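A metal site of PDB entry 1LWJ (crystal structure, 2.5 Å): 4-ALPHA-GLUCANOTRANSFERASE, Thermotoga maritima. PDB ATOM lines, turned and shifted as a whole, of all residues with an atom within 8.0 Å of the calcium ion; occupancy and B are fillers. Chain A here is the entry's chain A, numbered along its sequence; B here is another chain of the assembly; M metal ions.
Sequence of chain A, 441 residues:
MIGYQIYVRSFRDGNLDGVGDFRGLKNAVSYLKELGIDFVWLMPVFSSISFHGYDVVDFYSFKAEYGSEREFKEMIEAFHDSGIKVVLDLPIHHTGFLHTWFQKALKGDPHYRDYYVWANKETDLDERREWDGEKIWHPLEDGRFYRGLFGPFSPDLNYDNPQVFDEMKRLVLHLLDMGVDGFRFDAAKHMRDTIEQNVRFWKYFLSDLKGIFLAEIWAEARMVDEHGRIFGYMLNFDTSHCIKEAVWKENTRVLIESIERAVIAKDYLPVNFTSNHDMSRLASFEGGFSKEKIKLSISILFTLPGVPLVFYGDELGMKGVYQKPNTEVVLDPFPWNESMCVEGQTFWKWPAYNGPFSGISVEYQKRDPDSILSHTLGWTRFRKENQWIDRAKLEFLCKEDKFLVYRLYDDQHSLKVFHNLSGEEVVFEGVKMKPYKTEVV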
ATOM      1  N   ARG A   9      -6.831  21.663  19.484  1.00  0.00           N
ATOM      2  CA  ARG A   9      -5.879  22.168  20.489  1.00  0.00           C
ATOM      3  C   ARG A   9      -5.603  23.659  20.470  1.00  0.00           C
ATOM      4  O   ARG A   9      -5.188  24.224  21.484  1.00  0.00           O
ATOM      5  CB  ARG A   9      -4.538  21.436  20.375  1.00  0.00           C
ATOM      6  CG  ARG A   9      -3.537  21.752  21.493  1.00  0.00           C
ATOM      7  CD  ARG A   9      -2.145  21.229  21.153  1.00  0.00           C
ATOM      8  NE  ARG A   9      -1.955  19.801  21.377  1.00  0.00           N
ATOM      9  CZ  ARG A   9      -0.866  19.120  21.034  1.00  0.00           C
ATOM     10  NH1 ARG A   9       0.141  19.731  20.433  1.00  0.00           N
ATOM     11  NH2 ARG A   9      -0.757  17.827  21.309  1.00  0.00           N
ATOM     12  N   ARG A  12     -10.290  26.467  21.436  1.00  0.00           N
ATOM     13  CA  ARG A  12     -10.699  26.944  22.755  1.00  0.00           C
ATOM     14  C   ARG A  12     -10.537  25.903  23.895  1.00  0.00           C
ATOM     15  O   ARG A  12     -10.884  24.718  23.758  1.00  0.00           O
ATOM     16  CB  ARG A  12     -12.127  27.465  22.686  1.00  0.00           C
ATOM     17  CG  ARG A  12     -12.559  28.243  23.891  1.00  0.00           C
ATOM     18  CD  ARG A  12     -14.033  28.505  23.790  1.00  0.00           C
ATOM     19  NE  ARG A  12     -14.548  29.181  24.974  1.00  0.00           N
ATOM     20  CZ  ARG A  12     -14.571  30.496  25.142  1.00  0.00           C
ATOM     21  NH1 ARG A  12     -14.104  31.312  24.197  1.00  0.00           N
ATOM     22  NH2 ARG A  12     -15.063  31.011  26.270  1.00  0.00           N
ATOM     23  N   ASP A  13      -9.990  26.375  24.994  1.00  0.00           N
ATOM     24  CA  ASP A  13      -9.733  25.568  26.171  1.00  0.00           C
ATOM     25  C   ASP A  13     -10.940  25.639  27.104  1.00  0.00           C
ATOM     26  O   ASP A  13     -11.516  26.709  27.333  1.00  0.00           O
ATOM     27  CB  ASP A  13      -8.455  26.102  26.852  1.00  0.00           C
ATOM     28  CG  ASP A  13      -8.172  25.453  28.189  1.00  0.00           C
ATOM     29  OD1 ASP A  13      -8.158  24.201  28.277  1.00  0.00           O
ATOM     30  OD2 ASP A  13      -7.924  26.209  29.148  1.00  0.00           O
ATOM     31  N   GLY A  14     -11.340  24.483  27.633  1.00  0.00           N
ATOM     32  CA  GLY A  14     -12.501  24.470  28.487  1.00  0.00           C
ATOM     33  C   GLY A  14     -12.248  23.999  29.904  1.00  0.00           C
ATOM     34  O   GLY A  14     -13.179  23.986  30.703  1.00  0.00           O
ATOM     35  N   ASN A  15     -11.016  23.604  30.212  1.00  0.00           N
ATOM     36  CA  ASN A  15     -10.746  23.147  31.570  1.00  0.00           C
ATOM     37  C   ASN A  15      -9.561  23.846  32.215  1.00  0.00           C
ATOM     38  O   ASN A  15      -8.933  23.307  33.132  1.00  0.00           O
ATOM     39  CB  ASN A  15     -10.538  21.632  31.612  1.00  0.00           C
ATOM     40  CG  ASN A  15      -9.668  21.131  30.504  1.00  0.00           C
ATOM     41  OD1 ASN A  15      -8.788  21.843  30.028  1.00  0.00           O
ATOM     42  ND2 ASN A  15      -9.889  19.893  30.092  1.00  0.00           N
ATOM     43  N   LEU A  16      -9.272  25.045  31.740  1.00  0.00           N
ATOM     44  CA  LEU A  16      -8.201  25.896  32.274  1.00  0.00           C
ATOM     45  C   LEU A  16      -6.801  25.312  32.256  1.00  0.00           C
ATOM     46  O   LEU A  16      -6.163  25.225  33.306  1.00  0.00           O
ATOM     47  CB  LEU A  16      -8.544  26.317  33.712  1.00  0.00           C
ATOM     48  CG  LEU A  16      -9.916  26.944  33.947  1.00  0.00           C
ATOM     49  CD1 LEU A  16     -10.166  27.086  35.440  1.00  0.00           C
ATOM     50  CD2 LEU A  16     -10.016  28.285  33.205  1.00  0.00           C
ATOM     51  N   ASP A  17      -6.307  24.917  31.088  1.00  0.00           N
ATOM     52  CA  ASP A  17      -4.953  24.392  31.024  1.00  0.00           C
ATOM     53  C   ASP A  17      -4.218  24.928  29.790  1.00  0.00           C
ATOM     54  O   ASP A  17      -3.050  24.624  29.555  1.00  0.00           O
ATOM     55  CB  ASP A  17      -4.982  22.856  31.053  1.00  0.00           C
ATOM     56  CG  ASP A  17      -5.456  22.242  29.764  1.00  0.00           C
ATOM     57  OD1 ASP A  17      -6.193  22.919  29.014  1.00  0.00           O
ATOM     58  OD2 ASP A  17      -5.094  21.082  29.515  1.00  0.00           O
ATOM     59  N   GLY A  18      -4.927  25.755  29.020  1.00  0.00           N
ATOM     60  CA  GLY A  18      -4.320  26.342  27.832  1.00  0.00           C
ATOM     61  C   GLY A  18      -4.342  25.461  26.605  1.00  0.00           C
ATOM     62  O   GLY A  18      -3.940  25.894  25.524  1.00  0.00           O
ATOM     63  N   VAL A  19      -4.797  24.222  26.762  1.00  0.00           N
ATOM     64  CA  VAL A  19      -4.878  23.286  25.657  1.00  0.00           C
ATOM     65  C   VAL A  19      -6.327  23.178  25.168  1.00  0.00           C
ATOM     66  O   VAL A  19      -7.237  22.902  25.966  1.00  0.00           O
ATOM     67  CB  VAL A  19      -4.377  21.875  26.085  1.00  0.00           C
ATOM     68  CG1 VAL A  19      -4.176  20.960  24.853  1.00  0.00           C
ATOM     69  CG2 VAL A  19      -3.093  22.015  26.880  1.00  0.00           C
ATOM     70  N   GLY A  20      -6.543  23.418  23.873  1.00  0.00           N
ATOM     71  CA  GLY A  20      -7.888  23.338  23.312  1.00  0.00           C
ATOM     72  C   GLY A  20      -8.547  21.980  23.535  1.00  0.00           C
ATOM     73  O   GLY A  20      -7.918  20.937  23.344  1.00  0.00           O
ATOM     74  N   ASP A  21      -9.810  21.966  23.927  1.00  0.00           N
ATOM     75  CA  ASP A  21     -10.472  20.705  24.186  1.00  0.00           C
ATOM     76  C   ASP A  21     -11.941  20.711  23.798  1.00  0.00           C
ATOM     77  O   ASP A  21     -12.460  21.727  23.335  1.00  0.00           O
ATOM     78  CB  ASP A  21     -10.332  20.354  25.655  1.00  0.00           C
ATOM     79  CG  ASP A  21     -10.602  21.526  26.543  1.00  0.00           C
ATOM     80  OD1 ASP A  21     -11.736  22.040  26.496  1.00  0.00           O
ATOM     81  OD2 ASP A  21      -9.697  21.966  27.281  1.00  0.00           O
ATOM     82  N   PHE A  22     -12.601  19.587  24.031  1.00  0.00           N
ATOM     83  CA  PHE A  22     -14.010  19.432  23.693  1.00  0.00           C
ATOM     84  C   PHE A  22     -14.924  20.403  24.446  1.00  0.00           C
ATOM     85  O   PHE A  22     -15.852  20.956  23.865  1.00  0.00           O
ATOM     86  CB  PHE A  22     -14.474  17.992  23.946  1.00  0.00           C
ATOM     87  CG  PHE A  22     -13.825  16.963  23.050  1.00  0.00           C
ATOM     88  CD1 PHE A  22     -13.487  17.258  21.739  1.00  0.00           C
ATOM     89  CD2 PHE A  22     -13.566  15.677  23.519  1.00  0.00           C
ATOM     90  CE1 PHE A  22     -12.906  16.292  20.903  1.00  0.00           C
ATOM     91  CE2 PHE A  22     -12.993  14.701  22.689  1.00  0.00           C
ATOM     92  CZ  PHE A  22     -12.664  15.017  21.387  1.00  0.00           C
ATOM     93  N   ARG A  23     -14.660  20.605  25.741  1.00  0.00           N
ATOM     94  CA  ARG A  23     -15.476  21.529  26.525  1.00  0.00           C
ATOM     95  C   ARG A  23     -15.380  22.962  25.984  1.00  0.00           C
ATOM     96  O   ARG A  23     -16.396  23.626  25.807  1.00  0.00           O
ATOM     97  CB  ARG A  23     -15.093  21.476  28.016  1.00  0.00           C
ATOM     98  CG  ARG A  23     -15.635  20.248  28.755  1.00  0.00           C
ATOM     99  CD  ARG A  23     -15.158  20.189  30.187  1.00  0.00           C
ATOM    100  NE  ARG A  23     -15.466  21.428  30.892  1.00  0.00           N
ATOM    101  CZ  ARG A  23     -15.003  21.732  32.115  1.00  0.00           C
ATOM    102  NH1 ARG A  23     -14.207  20.879  32.757  1.00  0.00           N
ATOM    103  NH2 ARG A  23     -15.332  22.889  32.686  1.00  0.00           N
ATOM    104  N   GLY A  24     -14.176  23.426  25.718  1.00  0.00           N
ATOM    105  CA  GLY A  24     -14.013  24.764  25.181  1.00  0.00           C
ATOM    106  C   GLY A  24     -14.683  24.894  23.816  1.00  0.00           C
ATOM    107  O   GLY A  24     -15.282  25.918  23.495  1.00  0.00           O
ATOM    108  N   ALA A  64      -6.780  12.266  24.957  1.00  0.00           N
ATOM    109  CA  ALA A  64      -6.968  12.604  26.364  1.00  0.00           C
ATOM    110  C   ALA A  64      -6.941  14.101  26.628  1.00  0.00           C
ATOM    111  O   ALA A  64      -7.693  14.593  27.462  1.00  0.00           O
ATOM    112  CB  ALA A  64      -5.903  11.935  27.196  1.00  0.00           C
ATOM    113  N   GLU A  65      -6.064  14.812  25.921  1.00  0.00           N
ATOM    114  CA  GLU A  65      -5.936  16.256  26.099  1.00  0.00           C
ATOM    115  C   GLU A  65      -7.150  17.060  25.646  1.00  0.00           C
ATOM    116  O   GLU A  65      -7.367  18.195  26.094  1.00  0.00           O
ATOM    117  CB  GLU A  65      -4.690  16.737  25.370  1.00  0.00           C
ATOM    118  CG  GLU A  65      -4.525  16.137  23.994  1.00  0.00           C
ATOM    119  CD  GLU A  65      -3.745  17.048  23.073  1.00  0.00           C
ATOM    120  OE1 GLU A  65      -3.194  16.552  22.072  1.00  0.00           O
ATOM    121  OE2 GLU A  65      -3.705  18.271  23.341  1.00  0.00           O
ATOM    122  N   TYR A  66      -7.951  16.481  24.751  1.00  0.00           N
ATOM    123  CA  TYR A  66      -9.156  17.143  24.259  1.00  0.00           C
ATOM    124  C   TYR A  66     -10.299  16.807  25.197  1.00  0.00           C
ATOM    125  O   TYR A  66     -11.167  17.652  25.456  1.00  0.00           O
ATOM    126  CB  TYR A  66      -9.462  16.679  22.837  1.00  0.00           C
ATOM    127  CG  TYR A  66      -8.458  17.150  21.793  1.00  0.00           C
ATOM    128  CD1 TYR A  66      -8.519  16.684  20.482  1.00  0.00           C
ATOM    129  CD2 TYR A  66      -7.462  18.077  22.110  1.00  0.00           C
ATOM    130  CE1 TYR A  66      -7.633  17.129  19.514  1.00  0.00           C
ATOM    131  CE2 TYR A  66      -6.565  18.542  21.139  1.00  0.00           C
ATOM    132  CZ  TYR A  66      -6.656  18.058  19.842  1.00  0.00           C
ATOM    133  OH  TYR A  66      -5.783  18.505  18.878  1.00  0.00           O
ATOM    134  N   GLY A  67     -10.296  15.577  25.701  1.00  0.00           N
ATOM    135  CA  GLY A  67     -11.332  15.153  26.623  1.00  0.00           C
ATOM    136  C   GLY A  67     -11.699  13.682  26.622  1.00  0.00           C
ATOM    137  O   GLY A  67     -11.058  12.855  25.979  1.00  0.00           O
ATOM    138  N   THR A 346      -6.206  29.546  24.343  1.00  0.00           N
ATOM    139  CA  THR A 346      -5.241  28.441  24.313  1.00  0.00           C
ATOM    140  C   THR A 346      -3.851  29.068  24.300  1.00  0.00           C
ATOM    141  O   THR A 346      -3.693  30.233  23.938  1.00  0.00           O
ATOM    142  CB  THR A 346      -5.380  27.581  23.049  1.00  0.00           C
ATOM    143  OG1 THR A 346      -5.497  28.430  21.897  1.00  0.00           O
ATOM    144  CG2 THR A 346      -6.571  26.665  23.160  1.00  0.00           C
ATOM    145  N   SER B  48      -3.307  26.180  34.811  1.00  0.00           N
ATOM    146  CA  SER B  48      -2.792  27.451  34.301  1.00  0.00           C
ATOM    147  C   SER B  48      -2.958  27.379  32.788  1.00  0.00           C
ATOM    148  O   SER B  48      -3.089  26.297  32.254  1.00  0.00           O
ATOM    149  CB  SER B  48      -1.300  27.602  34.620  1.00  0.00           C
ATOM    150  OG  SER B  48      -0.715  28.596  33.801  1.00  0.00           O
ATOM    151  N   LYS B  63      -3.442  20.449  36.166  1.00  0.00           N
ATOM    152  CA  LYS B  63      -3.466  20.755  34.742  1.00  0.00           C
ATOM    153  C   LYS B  63      -4.164  19.657  33.933  1.00  0.00           C
ATOM    154  O   LYS B  63      -3.598  18.595  33.686  1.00  0.00           O
ATOM    155  CB  LYS B  63      -2.038  20.926  34.229  1.00  0.00           C
ATOM    156  CG  LYS B  63      -1.853  22.105  33.323  1.00  0.00           C
ATOM    157  CD  LYS B  63      -0.405  22.289  32.957  1.00  0.00           C
ATOM    158  CE  LYS B  63      -0.183  23.697  32.457  1.00  0.00           C
ATOM    159  NZ  LYS B  63      -1.037  24.022  31.278  1.00  0.00           N
ATOM    160  N   ALA B  64      -5.393  19.922  33.522  1.00  0.00           N
ATOM    161  CA  ALA B  64      -6.181  18.991  32.740  1.00  0.00           C
ATOM    162  C   ALA B  64      -5.401  17.959  31.915  1.00  0.00           C
ATOM    163  O   ALA B  64      -5.643  16.759  32.012  1.00  0.00           O
ATOM    164  CB  ALA B  64      -7.098  19.777  31.828  1.00  0.00           C
ATOM    165  N   GLU B  65      -4.462  18.458  31.109  1.00  0.00           N
ATOM    166  CA  GLU B  65      -3.623  17.632  30.234  1.00  0.00           C
ATOM    167  C   GLU B  65      -2.804  16.545  30.916  1.00  0.00           C
ATOM    168  O   GLU B  65      -2.585  15.466  30.357  1.00  0.00           O
ATOM    169  CB  GLU B  65      -2.683  18.537  29.440  1.00  0.00           C
ATOM    170  CG  GLU B  65      -2.091  19.659  30.256  1.00  0.00           C
ATOM    171  CD  GLU B  65      -1.006  20.394  29.508  1.00  0.00           C
ATOM    172  OE1 GLU B  65      -0.709  21.555  29.862  1.00  0.00           O
ATOM    173  OE2 GLU B  65      -0.427  19.795  28.570  1.00  0.00           O
HETATM  174 CA    CA M   1      -7.690  21.714  28.006  1.00  0.00          CA
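OD1 of Asp 21 sits at hydrogen-bond distance from N of Gly 14. The backbone NH of Asp 21 lies within hydrogen-bond range of the backbone carbonyl oxygen of Arg 12, 3.0 Å away. N of Gly 24 is in hydrogen-bond range of OD1 of Asp 21, at 2.9 Å. OD1 of Asp 21 lies within hydrogen-bond range of N of Arg 23 (3.3 Å). The side-chain carboxylate of Asp 17 sits at hydrogen-bond distance from the backbone NH of Glu 65 of chain B (3.1 Å). O of Asp 17 lies within hydrogen-bond range of NZ of Lys 63 of chain B, 2.7 Å away. The side-chain carboxylate (OD2) of Asp 13 sits at hydrogen-bond distance from the backbone NH (N) of Gly 18, 3.0 Å away. OD2 of Asp 13 is in hydrogen-bond range of N of Leu 16 (3.1 Å).
Of the 23 residues printed, 5 come within 4 Å of the calcium ion. The nearest printed residue that does not touch the calcium ion is Glu 65 of chain A (4.02 Å).
The calcium ion is bound by OD2 of Asp 21 (2.1 Å). The side-chain carboxylate (OD1) of Asp 17 is bound to the calcium ion. The side-chain amide oxygen (OD1) of Asn 15 binds the calcium ion. O of Val 19 is bound to the calcium ion. OD1 of Asp 13 is bound to the calcium ion (2.5 Å). The calcium ion has five donor atoms within binding distance. Slightly farther from the calcium ion lies the side-chain carboxylate (OD2) of Asp 17 (3.1 Å).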
